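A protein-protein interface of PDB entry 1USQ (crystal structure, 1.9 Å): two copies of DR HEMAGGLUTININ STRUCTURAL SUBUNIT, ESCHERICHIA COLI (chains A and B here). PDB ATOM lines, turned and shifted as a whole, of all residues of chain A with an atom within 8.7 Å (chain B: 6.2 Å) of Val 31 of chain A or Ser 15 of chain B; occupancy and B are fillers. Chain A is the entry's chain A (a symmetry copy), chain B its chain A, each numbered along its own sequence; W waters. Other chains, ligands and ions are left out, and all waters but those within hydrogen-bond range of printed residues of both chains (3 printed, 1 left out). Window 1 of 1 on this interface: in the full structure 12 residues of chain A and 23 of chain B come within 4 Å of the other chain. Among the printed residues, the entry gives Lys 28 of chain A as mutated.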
ATOM      1  N   THR A  24      27.201  25.581  19.804  1.00  0.00           N
ATOM      2  CA  THR A  24      25.965  24.988  20.234  1.00  0.00           C
ATOM      3  C   THR A  24      25.491  25.742  21.464  1.00  0.00           C
ATOM      4  O   THR A  24      26.249  25.919  22.426  1.00  0.00           O
ATOM      5  CB  THR A  24      26.118  23.502  20.537  1.00  0.00           C
ATOM      6  OG1 THR A  24      26.346  22.791  19.313  1.00  0.00           O
ATOM      7  CG2 THR A  24      24.849  22.980  21.223  1.00  0.00           C
ATOM      8  N   VAL A  25      24.290  26.304  21.368  1.00  0.00           N
ATOM      9  CA  VAL A  25      23.685  27.063  22.471  1.00  0.00           C
ATOM     10  C   VAL A  25      22.755  26.112  23.243  1.00  0.00           C
ATOM     11  O   VAL A  25      22.057  25.292  22.647  1.00  0.00           O
ATOM     12  CB  VAL A  25      22.849  28.243  21.932  1.00  0.00           C
ATOM     13  CG1 VAL A  25      22.081  28.919  23.053  1.00  0.00           C
ATOM     14  CG2 VAL A  25      23.745  29.245  21.222  1.00  0.00           C
ATOM     15  N   THR A  26      22.775  26.215  24.571  1.00  0.00           N
ATOM     16  CA  THR A  26      21.985  25.327  25.413  1.00  0.00           C
ATOM     17  C   THR A  26      21.310  26.118  26.519  1.00  0.00           C
ATOM     18  O   THR A  26      21.480  27.327  26.618  1.00  0.00           O
ATOM     19  CB  THR A  26      22.874  24.244  26.085  1.00  0.00           C
ATOM     20  OG1 THR A  26      23.540  24.806  27.220  1.00  0.00           O
ATOM     21  CG2 THR A  26      23.939  23.667  25.093  1.00  0.00           C
ATOM     22  N   GLU A  27      20.578  25.411  27.373  1.00  0.00           N
ATOM     23  CA  GLU A  27      19.989  25.992  28.574  1.00  0.00           C
ATOM     24  C   GLU A  27      21.028  25.820  29.683  1.00  0.00           C
ATOM     25  O   GLU A  27      22.124  25.282  29.439  1.00  0.00           O
ATOM     26  CB  GLU A  27      18.710  25.231  28.959  1.00  0.00           C
ATOM     27  CG  GLU A  27      17.587  25.367  27.944  1.00  0.00           C
ATOM     28  CD  GLU A  27      16.234  25.156  28.558  1.00  0.00           C
ATOM     29  OE1 GLU A  27      16.170  24.839  29.768  1.00  0.00           O
ATOM     30  OE2 GLU A  27      15.229  25.318  27.836  1.00  0.00           O
ATOM     31  N   LYS A  28      20.657  26.206  30.904  1.00  0.00           N
ATOM     32  CA  LYS A  28      21.535  26.048  32.059  1.00  0.00           C
ATOM     33  C   LYS A  28      21.840  24.566  32.316  1.00  0.00           C
ATOM     34  O   LYS A  28      22.992  24.216  32.557  1.00  0.00           O
ATOM     35  CB  LYS A  28      20.930  26.717  33.301  1.00  0.00           C
ATOM     36  CG  LYS A  28      21.777  26.628  34.558  1.00  0.00           C
ATOM     37  CD  LYS A  28      20.899  26.732  35.797  1.00  0.00           C
ATOM     38  CE  LYS A  28      20.492  25.361  36.305  1.00  0.00           C
ATOM     39  NZ  LYS A  28      21.565  24.731  37.108  1.00  0.00           N
ATOM     40  N   CYS A  29      20.835  23.694  32.171  1.00  0.00           N
ATOM     41  CA  CYS A  29      21.066  22.243  32.264  1.00  0.00           C
ATOM     42  C   CYS A  29      21.512  21.820  30.875  1.00  0.00           C
ATOM     43  O   CYS A  29      20.740  21.880  29.922  1.00  0.00           O
ATOM     44  CB  CYS A  29      19.813  21.474  32.694  1.00  0.00           C
ATOM     45  SG  CYS A  29      19.887  19.660  32.421  1.00  0.00           S
ATOM     46  N   GLN A  30      22.802  21.488  30.773  1.00  0.00           N
ATOM     47  CA  GLN A  30      23.491  21.279  29.509  1.00  0.00           C
ATOM     48  C   GLN A  30      24.071  19.870  29.458  1.00  0.00           C
ATOM     49  O   GLN A  30      24.860  19.487  30.311  1.00  0.00           O
ATOM     50  CB  GLN A  30      24.617  22.310  29.422  1.00  0.00           C
ATOM     51  CG  GLN A  30      25.644  22.118  28.335  1.00  0.00           C
ATOM     52  CD  GLN A  30      26.773  23.117  28.478  1.00  0.00           C
ATOM     53  OE1 GLN A  30      27.699  22.888  29.253  1.00  0.00           O
ATOM     54  NE2 GLN A  30      26.566  24.322  27.947  1.00  0.00           N
ATOM     55  N   VAL A  31      23.681  19.113  28.435  1.00  0.00           N
ATOM     56  CA  VAL A  31      24.119  17.721  28.298  1.00  0.00           C
ATOM     57  C   VAL A  31      25.040  17.497  27.084  1.00  0.00           C
ATOM     58  O   VAL A  31      24.598  17.441  25.945  1.00  0.00           O
ATOM     59  CB  VAL A  31      22.912  16.769  28.275  1.00  0.00           C
ATOM     60  CG1 VAL A  31      23.377  15.293  28.297  1.00  0.00           C
ATOM     61  CG2 VAL A  31      22.002  17.071  29.492  1.00  0.00           C
ATOM     62  N   ARG A  32      26.337  17.411  27.357  1.00  0.00           N
ATOM     63  CA  ARG A  32      27.334  17.249  26.315  1.00  0.00           C
ATOM     64  C   ARG A  32      27.473  15.782  25.974  1.00  0.00           C
ATOM     65  O   ARG A  32      27.817  14.976  26.827  1.00  0.00           O
ATOM     66  CB  ARG A  32      28.675  17.810  26.782  1.00  0.00           C
ATOM     67  CG  ARG A  32      28.619  19.298  27.104  1.00  0.00           C
ATOM     68  CD  ARG A  32      29.920  19.799  27.650  1.00  0.00           C
ATOM     69  NE  ARG A  32      29.848  21.228  27.943  1.00  0.00           N
ATOM     70  CZ  ARG A  32      30.507  22.157  27.263  1.00  0.00           C
ATOM     71  NH1 ARG A  32      31.279  21.809  26.236  1.00  0.00           N
ATOM     72  NH2 ARG A  32      30.384  23.438  27.604  1.00  0.00           N
ATOM     73  N   VAL A  33      27.257  15.472  24.707  1.00  0.00           N
ATOM     74  CA  VAL A  33      27.261  14.109  24.188  1.00  0.00           C
ATOM     75  C   VAL A  33      28.351  13.973  23.129  1.00  0.00           C
ATOM     76  O   VAL A  33      28.408  14.745  22.161  1.00  0.00           O
ATOM     77  CB  VAL A  33      25.864  13.755  23.537  1.00  0.00           C
ATOM     78  CG1 VAL A  33      25.827  12.297  23.066  1.00  0.00           C
ATOM     79  CG2 VAL A  33      24.715  14.035  24.539  1.00  0.00           C
ATOM     80  N   GLY A  34      29.226  13.005  23.317  1.00  0.00           N
ATOM     81  CA  GLY A  34      30.333  12.804  22.396  1.00  0.00           C
ATOM     82  C   GLY A  34      31.474  13.803  22.634  1.00  0.00           C
ATOM     83  O   GLY A  34      31.590  14.412  23.712  1.00  0.00           O
ATOM     84  N   THR A  37      32.953  20.052  21.826  1.00  0.00           N
ATOM     85  CA  THR A  37      32.710  21.042  20.792  1.00  0.00           C
ATOM     86  C   THR A  37      32.463  22.334  21.544  1.00  0.00           C
ATOM     87  O   THR A  37      32.323  22.330  22.767  1.00  0.00           O
ATOM     88  CB  THR A  37      31.449  20.722  19.948  1.00  0.00           C
ATOM     89  OG1 THR A  37      30.306  20.628  20.815  1.00  0.00           O
ATOM     90  CG2 THR A  37      31.626  19.401  19.173  1.00  0.00           C
ATOM     91  N   ALA A  39      30.414  25.033  23.095  1.00  0.00           N
ATOM     92  CA  ALA A  39      29.046  25.116  23.578  1.00  0.00           C
ATOM     93  C   ALA A  39      28.952  26.162  24.665  1.00  0.00           C
ATOM     94  O   ALA A  39      29.871  26.320  25.464  1.00  0.00           O
ATOM     95  CB  ALA A  39      28.591  23.752  24.121  1.00  0.00           C
ATOM     96  N   LYS A  40      27.838  26.877  24.688  1.00  0.00           N
ATOM     97  CA  LYS A  40      27.572  27.871  25.725  1.00  0.00           C
ATOM     98  C   LYS A  40      26.098  27.823  26.081  1.00  0.00           C
ATOM     99  O   LYS A  40      25.265  27.497  25.243  1.00  0.00           O
ATOM    100  CB  LYS A  40      27.898  29.280  25.214  1.00  0.00           C
ATOM    101  CG  LYS A  40      29.386  29.554  25.038  1.00  0.00           C
ATOM    102  CD  LYS A  40      29.621  30.918  24.417  1.00  0.00           C
ATOM    103  CE  LYS A  40      31.107  31.236  24.351  1.00  0.00           C
ATOM    104  NZ  LYS A  40      31.352  32.693  24.393  1.00  0.00           N
ATOM    105  N   THR A  41      25.778  28.177  27.324  1.00  0.00           N
ATOM    106  CA  THR A  41      24.398  28.343  27.733  1.00  0.00           C
ATOM    107  C   THR A  41      23.949  29.684  27.156  1.00  0.00           C
ATOM    108  O   THR A  41      24.780  30.517  26.823  1.00  0.00           O
ATOM    109  CB  THR A  41      24.286  28.374  29.277  1.00  0.00           C
ATOM    110  OG1 THR A  41      24.896  29.573  29.775  1.00  0.00           O
ATOM    111  CG2 THR A  41      25.014  27.169  29.876  1.00  0.00           C
ATOM    112  N   ARG A  42      22.651  29.880  26.961  1.00  0.00           N
ATOM    113  CA  ARG A  42      22.210  31.155  26.387  1.00  0.00           C
ATOM    114  C   ARG A  42      22.556  32.323  27.310  1.00  0.00           C
ATOM    115  O   ARG A  42      22.804  33.438  26.856  1.00  0.00           O
ATOM    116  CB  ARG A  42      20.724  31.140  26.044  1.00  0.00           C
ATOM    117  CG  ARG A  42      19.874  30.396  27.014  1.00  0.00           C
ATOM    118  CD  ARG A  42      18.491  30.157  26.451  1.00  0.00           C
ATOM    119  NE  ARG A  42      17.532  29.929  27.518  1.00  0.00           N
ATOM    120  CZ  ARG A  42      16.241  29.679  27.339  1.00  0.00           C
ATOM    121  NH1 ARG A  42      15.731  29.595  26.118  1.00  0.00           N
ATOM    122  NH2 ARG A  42      15.459  29.505  28.393  1.00  0.00           N
ATOM    123  N   PRO A 134      17.450  30.750  21.165  1.00  0.00           N
ATOM    124  CA  PRO A 134      16.928  29.385  21.256  1.00  0.00           C
ATOM    125  C   PRO A 134      18.069  28.358  21.193  1.00  0.00           C
ATOM    126  O   PRO A 134      18.991  28.489  20.386  1.00  0.00           O
ATOM    127  CB  PRO A 134      16.049  29.259  20.004  1.00  0.00           C
ATOM    128  CG  PRO A 134      15.732  30.669  19.612  1.00  0.00           C
ATOM    129  CD  PRO A 134      16.913  31.477  20.000  1.00  0.00           C
ATOM    130  N   PRO A 135      17.993  27.321  22.017  1.00  0.00           N
ATOM    131  CA  PRO A 135      19.037  26.307  22.006  1.00  0.00           C
ATOM    132  C   PRO A 135      19.076  25.625  20.641  1.00  0.00           C
ATOM    133  O   PRO A 135      18.039  25.379  20.031  1.00  0.00           O
ATOM    134  CB  PRO A 135      18.575  25.332  23.089  1.00  0.00           C
ATOM    135  CG  PRO A 135      17.862  26.212  24.070  1.00  0.00           C
ATOM    136  CD  PRO A 135      17.154  27.233  23.233  1.00  0.00           C
ATOM    137  N   GLY A 136      20.279  25.426  20.115  1.00  0.00           N
ATOM    138  CA  GLY A 136      20.439  24.791  18.812  1.00  0.00           C
ATOM    139  C   GLY A 136      21.903  24.883  18.405  1.00  0.00           C
ATOM    140  O   GLY A 136      22.761  25.249  19.219  1.00  0.00           O
ATOM    141  N   ASN A 137      22.182  24.468  17.172  1.00  0.00           N
ATOM    142  CA  ASN A 137      23.525  24.507  16.605  1.00  0.00           C
ATOM    143  C   ASN A 137      23.589  25.649  15.627  1.00  0.00           C
ATOM    144  O   ASN A 137      22.749  25.765  14.730  1.00  0.00           O
ATOM    145  CB  ASN A 137      23.832  23.200  15.870  1.00  0.00           C
ATOM    146  CG  ASN A 137      23.612  21.994  16.736  1.00  0.00           C
ATOM    147  OD1 ASN A 137      24.148  21.917  17.836  1.00  0.00           O
ATOM    148  ND2 ASN A 137      22.669  21.157  16.341  1.00  0.00           N
ATOM    149  N   PHE B  12      10.816  16.080  26.113  1.00  0.00           N
ATOM    150  CA  PHE B  12      12.261  16.284  25.993  1.00  0.00           C
ATOM    151  C   PHE B  12      12.550  17.730  25.597  1.00  0.00           C
ATOM    152  O   PHE B  12      11.950  18.259  24.664  1.00  0.00           O
ATOM    153  CB  PHE B  12      12.846  15.352  24.925  1.00  0.00           C
ATOM    154  CG  PHE B  12      14.299  15.607  24.629  1.00  0.00           C
ATOM    155  CD1 PHE B  12      14.690  16.289  23.470  1.00  0.00           C
ATOM    156  CD2 PHE B  12      15.289  15.162  25.504  1.00  0.00           C
ATOM    157  CE1 PHE B  12      16.038  16.493  23.190  1.00  0.00           C
ATOM    158  CE2 PHE B  12      16.630  15.389  25.237  1.00  0.00           C
ATOM    159  CZ  PHE B  12      17.007  16.042  24.080  1.00  0.00           C
ATOM    160  N   THR B  13      13.477  18.356  26.302  1.00  0.00           N
ATOM    161  CA  THR B  13      13.916  19.709  25.972  1.00  0.00           C
ATOM    162  C   THR B  13      15.357  19.589  25.456  1.00  0.00           C
ATOM    163  O   THR B  13      16.261  19.232  26.224  1.00  0.00           O
ATOM    164  CB  THR B  13      13.959  20.609  27.244  1.00  0.00           C
ATOM    165  OG1 THR B  13      12.643  20.757  27.788  1.00  0.00           O
ATOM    166  CG2 THR B  13      14.506  21.978  26.899  1.00  0.00           C
ATOM    167  N   PRO B  14      15.583  19.884  24.167  1.00  0.00           N
ATOM    168  CA  PRO B  14      16.951  19.810  23.636  1.00  0.00           C
ATOM    169  C   PRO B  14      17.819  20.842  24.354  1.00  0.00           C
ATOM    170  O   PRO B  14      17.466  22.028  24.442  1.00  0.00           O
ATOM    171  CB  PRO B  14      16.781  20.178  22.151  1.00  0.00           C
ATOM    172  CG  PRO B  14      15.355  19.874  21.838  1.00  0.00           C
ATOM    173  CD  PRO B  14      14.592  20.159  23.109  1.00  0.00           C
ATOM    174  N   SER B  15      18.944  20.389  24.890  1.00  0.00           N
ATOM    175  CA  SER B  15      19.845  21.279  25.607  1.00  0.00           C
ATOM    176  C   SER B  15      21.170  20.572  25.852  1.00  0.00           C
ATOM    177  O   SER B  15      21.344  19.888  26.853  1.00  0.00           O
ATOM    178  CB  SER B  15      19.218  21.714  26.939  1.00  0.00           C
ATOM    179  OG  SER B  15      20.089  22.562  27.644  1.00  0.00           O
ATOM    180  N   GLY B  16      22.065  20.660  24.871  1.00  0.00           N
ATOM    181  CA  GLY B  16      23.320  19.947  24.937  1.00  0.00           C
ATOM    182  C   GLY B  16      23.822  19.733  23.522  1.00  0.00           C
ATOM    183  O   GLY B  16      23.259  20.283  22.559  1.00  0.00           O
ATOM    184  N   THR B  17      24.864  18.915  23.393  1.00  0.00           N
ATOM    185  CA  THR B  17      25.470  18.650  22.097  1.00  0.00           C
ATOM    186  C   THR B  17      25.066  17.283  21.525  1.00  0.00           C
ATOM    187  O   THR B  17      24.309  16.532  22.142  1.00  0.00           O
ATOM    188  CB  THR B  17      26.985  18.778  22.161  1.00  0.00           C
ATOM    189  OG1 THR B  17      27.524  17.792  23.061  1.00  0.00           O
ATOM    190  CG2 THR B  17      27.360  20.179  22.627  1.00  0.00           C
ATOM    191  N   THR B  18      25.563  16.986  20.332  1.00  0.00           N
ATOM    192  CA  THR B  18      25.174  15.780  19.611  1.00  0.00           C
ATOM    193  C   THR B  18      26.318  14.789  19.447  1.00  0.00           C
ATOM    194  O   THR B  18      27.444  15.154  19.088  1.00  0.00           O
ATOM    195  CB  THR B  18      24.580  16.141  18.232  1.00  0.00           C
ATOM    196  OG1 THR B  18      23.445  16.984  18.424  1.00  0.00           O
ATOM    197  CG2 THR B  18      24.150  14.876  17.442  1.00  0.00           C
ATOM    198  N   VAL B  56      28.817  11.042  27.901  1.00  0.00           N
ATOM    199  CA  VAL B  56      27.802  11.987  28.324  1.00  0.00           C
ATOM    200  C   VAL B  56      28.337  12.698  29.540  1.00  0.00           C
ATOM    201  O   VAL B  56      28.852  12.070  30.465  1.00  0.00           O
ATOM    202  CB  VAL B  56      26.484  11.258  28.716  1.00  0.00           C
ATOM    203  CG1 VAL B  56      25.427  12.280  29.210  1.00  0.00           C
ATOM    204  CG2 VAL B  56      25.952  10.436  27.547  1.00  0.00           C
ATOM    205  N   GLN B  57      28.276  14.020  29.506  1.00  0.00           N
ATOM    206  CA  GLN B  57      28.736  14.839  30.606  1.00  0.00           C
ATOM    207  C   GLN B  57      27.730  15.967  30.765  1.00  0.00           C
ATOM    208  O   GLN B  57      27.620  16.832  29.904  1.00  0.00           O
ATOM    209  CB  GLN B  57      30.126  15.417  30.307  1.00  0.00           C
ATOM    210  CG  GLN B  57      31.236  14.376  30.293  1.00  0.00           C
ATOM    211  CD  GLN B  57      31.682  13.992  31.679  1.00  0.00           C
ATOM    212  OE1 GLN B  57      31.118  14.447  32.665  1.00  0.00           O
ATOM    213  NE2 GLN B  57      32.748  13.211  31.765  1.00  0.00           N
ATOM    214  N   ALA B  58      26.953  15.912  31.836  1.00  0.00           N
ATOM    215  CA  ALA B  58      25.948  16.938  32.119  1.00  0.00           C
ATOM    216  C   ALA B  58      26.467  17.956  33.128  1.00  0.00           C
ATOM    217  O   ALA B  58      27.260  17.625  34.025  1.00  0.00           O
ATOM    218  CB  ALA B  58      24.644  16.278  32.649  1.00  0.00           C
ATOM    219  N   LEU B  59      26.027  19.198  32.953  1.00  0.00           N
ATOM    220  CA  LEU B  59      26.390  20.312  33.832  1.00  0.00           C
ATOM    221  C   LEU B  59      25.134  21.157  34.061  1.00  0.00           C
ATOM    222  O   LEU B  59      24.381  21.407  33.122  1.00  0.00           O
ATOM    223  CB  LEU B  59      27.454  21.209  33.166  1.00  0.00           C
ATOM    224  CG  LEU B  59      28.829  20.606  32.902  1.00  0.00           C
ATOM    225  CD1 LEU B  59      28.953  20.090  31.460  1.00  0.00           C
ATOM    226  CD2 LEU B  59      29.925  21.600  33.223  1.00  0.00           C
ATOM    227  N   CYS B  61      22.491  20.378  35.863  1.00  0.00           N
ATOM    228  CA  CYS B  61      21.268  19.549  35.866  1.00  0.00           C
ATOM    229  C   CYS B  61      20.938  18.920  37.232  1.00  0.00           C
ATOM    230  O   CYS B  61      20.303  17.877  37.308  1.00  0.00           O
ATOM    231  CB  CYS B  61      21.361  18.447  34.787  1.00  0.00           C
ATOM    232  SG  CYS B  61      21.718  19.104  33.113  1.00  0.00           S
ATOM    233  N   VAL B  66      18.580  14.085  33.139  1.00  0.00           N
ATOM    234  CA  VAL B  66      19.395  14.064  31.928  1.00  0.00           C
ATOM    235  C   VAL B  66      18.764  13.127  30.912  1.00  0.00           C
ATOM    236  O   VAL B  66      18.157  12.115  31.282  1.00  0.00           O
ATOM    237  CB  VAL B  66      20.833  13.618  32.261  1.00  0.00           C
ATOM    238  CG1 VAL B  66      21.577  13.123  31.005  1.00  0.00           C
ATOM    239  CG2 VAL B  66      21.574  14.759  32.953  1.00  0.00           C
ATOM    240  N   ALA B  67      18.866  13.486  29.636  1.00  0.00           N
ATOM    241  CA  ALA B  67      18.255  12.688  28.578  1.00  0.00           C
ATOM    242  C   ALA B  67      18.988  12.798  27.242  1.00  0.00           C
ATOM    243  O   ALA B  67      19.655  13.808  26.951  1.00  0.00           O
ATOM    244  CB  ALA B  67      16.759  13.081  28.401  1.00  0.00           C
ATOM    245  N   LEU B  68      18.804  11.775  26.411  1.00  0.00           N
ATOM    246  CA  LEU B  68      19.336  11.746  25.064  1.00  0.00           C
ATOM    247  C   LEU B  68      18.177  11.436  24.145  1.00  0.00           C
ATOM    248  O   LEU B  68      17.420  10.500  24.388  1.00  0.00           O
ATOM    249  CB  LEU B  68      20.381  10.629  24.908  1.00  0.00           C
ATOM    250  CG  LEU B  68      21.614  10.645  25.818  1.00  0.00           C
ATOM    251  CD1 LEU B  68      22.507  11.820  25.506  1.00  0.00           C
ATOM    252  CD2 LEU B  68      21.189  10.666  27.281  1.00  0.00           C
ATOM    253  N   TRP B 118      24.492  14.002  35.770  1.00  0.00           N
ATOM    254  CA  TRP B 118      25.184  12.739  35.505  1.00  0.00           C
ATOM    255  C   TRP B 118      26.272  12.877  34.430  1.00  0.00           C
ATOM    256  O   TRP B 118      26.103  13.570  33.413  1.00  0.00           O
ATOM    257  CB  TRP B 118      24.162  11.674  35.073  1.00  0.00           C
ATOM    258  CG  TRP B 118      24.710  10.261  34.881  1.00  0.00           C
ATOM    259  CD1 TRP B 118      25.023   9.367  35.858  1.00  0.00           C
ATOM    260  CD2 TRP B 118      24.951   9.580  33.623  1.00  0.00           C
ATOM    261  NE1 TRP B 118      25.402   8.166  35.302  1.00  0.00           N
ATOM    262  CE2 TRP B 118      25.359   8.265  33.934  1.00  0.00           C
ATOM    263  CE3 TRP B 118      24.812   9.942  32.277  1.00  0.00           C
ATOM    264  CZ2 TRP B 118      25.653   7.313  32.948  1.00  0.00           C
ATOM    265  CZ3 TRP B 118      25.124   8.998  31.294  1.00  0.00           C
ATOM    266  CH2 TRP B 118      25.547   7.700  31.642  1.00  0.00           C
ATOM    267  N   THR B 143      21.029  13.378  20.691  1.00  0.00           N
ATOM    268  CA  THR B 143      21.178  14.774  21.135  1.00  0.00           C
ATOM    269  C   THR B 143      20.912  14.914  22.632  1.00  0.00           C
ATOM    270  O   THR B 143      19.931  14.368  23.145  1.00  0.00           O
ATOM    271  CB  THR B 143      20.179  15.692  20.390  1.00  0.00           C
ATOM    272  OG1 THR B 143      20.412  15.604  18.984  1.00  0.00           O
ATOM    273  CG2 THR B 143      20.343  17.115  20.831  1.00  0.00           C
ATOM    274  N   GLY B 144      21.772  15.668  23.318  1.00  0.00           N
ATOM    275  CA  GLY B 144      21.643  15.871  24.769  1.00  0.00           C
ATOM    276  C   GLY B 144      20.538  16.863  25.146  1.00  0.00           C
ATOM    277  O   GLY B 144      20.247  17.807  24.412  1.00  0.00           O
ATOM    278  N   GLY B 145      19.929  16.639  26.305  1.00  0.00           N
ATOM    279  CA  GLY B 145      18.893  17.532  26.807  1.00  0.00           C
ATOM    280  C   GLY B 145      18.359  16.993  28.126  1.00  0.00           C
ATOM    281  O   GLY B 145      19.056  16.268  28.845  1.00  0.00           O
ATOM    282  N   TYR B 146      17.137  17.369  28.464  1.00  0.00           N
ATOM    283  CA  TYR B 146      16.546  16.891  29.707  1.00  0.00           C
ATOM    284  C   TYR B 146      15.068  16.572  29.565  1.00  0.00           C
ATOM    285  O   TYR B 146      14.396  17.087  28.676  1.00  0.00           O
ATOM    286  CB  TYR B 146      16.813  17.846  30.862  1.00  0.00           C
ATOM    287  CG  TYR B 146      16.269  19.231  30.665  1.00  0.00           C
ATOM    288  CD1 TYR B 146      17.056  20.240  30.107  1.00  0.00           C
ATOM    289  CD2 TYR B 146      14.982  19.550  31.079  1.00  0.00           C
ATOM    290  CE1 TYR B 146      16.578  21.532  29.981  1.00  0.00           C
ATOM    291  CE2 TYR B 146      14.489  20.834  30.960  1.00  0.00           C
ATOM    292  CZ  TYR B 146      15.290  21.825  30.412  1.00  0.00           C
ATOM    293  OH  TYR B 146      14.793  23.103  30.303  1.00  0.00           O
HETATM  294  O   HOH W   1      30.120  18.345  22.521  1.00  0.00           O
HETATM  295  O   HOH W   2      25.378  19.515  18.629  1.00  0.00           O
HETATM  296  O   HOH W   3      29.813  15.836  20.026  1.00  0.00           O
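No position is printed for both chains.
Water W3 lies within hydrogen-bond range of O of Thr 18 of chain B (2.6 Å) and O of Val 33 of chain A (2.8 Å).
Water W1 bridges OG1 of Thr 17 of chain B and OG1 of Thr 37 of chain A.
Water W2 lies within hydrogen-bond range of the side-chain amide oxygen of Asn 137 of chain A, the backbone NH of Thr 18 of chain B and the side-chain hydroxyl of Thr 24 of chain A.
Val 31 of chain A touches eight residues of chain B.
Of chain A, only Thr 26 (3.6 Å), Glu 27 (2.9 Å), Cys 29 (2.5 Å), Gln 30 (3.7 Å) and Val 31 (2.9 Å) come within 4 Å of Ser 15 of chain B.
Printed residues of chain A within 4 Å of Gly 16 of chain B: Thr 24 (3.4 Å), Thr 26 (3.6 Å) and Val 31 (3.0 Å).
Gly 144 of chain B touches just these residues of chain A: Val 31 (3.5 Å) and Val 33 (3.6 Å).
Gly 145 of chain B touches just one residue of chain A: Val 31 (3.1 Å).
Of the printed residues of chain B, Pro 135 of chain A touches Pro 14.
Printed residues of chain A within 4 Å of Thr 18 of chain B: Val 33 (3.2 Å).
Of the printed residues of chain A, Val 66 of chain B touches Val 31 (3.9 Å).
Of the printed residues of chain A, Val 56 of chain B touches Val 31 and Arg 32.
The nearest printed residue of chain B that does not touch Val 31 of chain A is Cys 61 of chain B (4.2 Å).
The side-chain hydroxyl of Ser 15 of chain B sits at hydrogen-bond distance from the backbone NH of Glu 27 of chain A (2.9 Å).
O of Cys 29 of chain A lies within hydrogen-bond range of OG of Ser 15 of chain B (2.5 Å).
The backbone carbonyl oxygen (O) of Ser 15 of chain B lies within hydrogen-bond range of the backbone NH (N) of Val 31 of chain A, at 2.9 Å.
The backbone NH of Thr 17 of chain B lies within hydrogen-bond range of the backbone carbonyl oxygen of Val 31 of chain A.
OG1 of Thr 17 of chain B sits at hydrogen-bond distance from N of Val 33 of chain A (2.9 Å).
The backbone NH (N) of Gln 57 of chain B is in hydrogen-bond range of the backbone carbonyl oxygen (O) of Arg 32 of chain A.
O of Leu 59 of chain B sits at hydrogen-bond distance from N of Gln 30 of chain A (2.8 Å).
The side-chain sulfur (SG) of Cys 61 of chain B is disulfide-bonded to the side-chain sulfur (SG) of Cys 29 of chain A (2.0 Å).
The side-chain sulfur (SG) of Cys 61 of chain B sits at hydrogen-bond distance from the backbone NH (N) of Gln 30 of chain A, at 3.5 Å.
OE2 of Glu 27 of chain A sits close to OH of Tyr 146 of chain B (3.3 Å).
The backbone carbonyl oxygen (O) of Leu 59 of chain B sits close to the backbone carbonyl oxygen (O) of Lys 28 of chain A (3.2 Å).
The backbone carbonyl oxygen of Thr 18 of chain B sits close to the backbone carbonyl oxygen of Val 33 of chain A (3.2 Å).
N of Thr 13 of chain B lies within hydrogen-bond range of O of Tyr 146 of chain B (2.8 Å).
The side-chain hydroxyl (OG1) of Thr 24 of chain A lies within hydrogen-bond range of the side-chain amide oxygen (OD1) of Asn 137 of chain A (2.8 Å).
The backbone NH of Arg 42 of chain A sits at hydrogen-bond distance from the backbone carbonyl oxygen of Thr 26 of chain A.
Of the 20 printed residues of chain A, 11 touch a printed residue of chain B.
Hydrophobic or aromatic side chains of chain A that line the printed part of chain B: Val 31, Val 33 and Pro 135.
Hydrophobic or aromatic side chains of chain B within 4 Å of the printed part of chain A: Val 56, Ala 58, Leu 59, Val 66, Leu 68 and Tyr 146.
Among the printed residues, no Asp or Glu carboxylate lies within 4 Å of a Lys or Arg side-chain nitrogen of the other chain.
CA of Cys 29 of chain A touches O of Leu 59 of chain B, 3.5 Å away.
Ser 15 of chain B touches Gln 30 of chain A (O to CA, 3.7 Å).
Gln 30 of chain A touches Ala 58 of chain B.
Val 56 of chain B touches Val 31 of chain A.
Val 31 of chain A touches Gly 144 of chain B.
CA of Val 56 of chain B touches O of Arg 32 of chain A, 3.3 Å away.
CG2 of Val 33 of chain A touches CD1 of Leu 68 of chain B (3.3 Å).
Pro 135 of chain A touches Pro 14 of chain B (CB to O, 3.7 Å).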
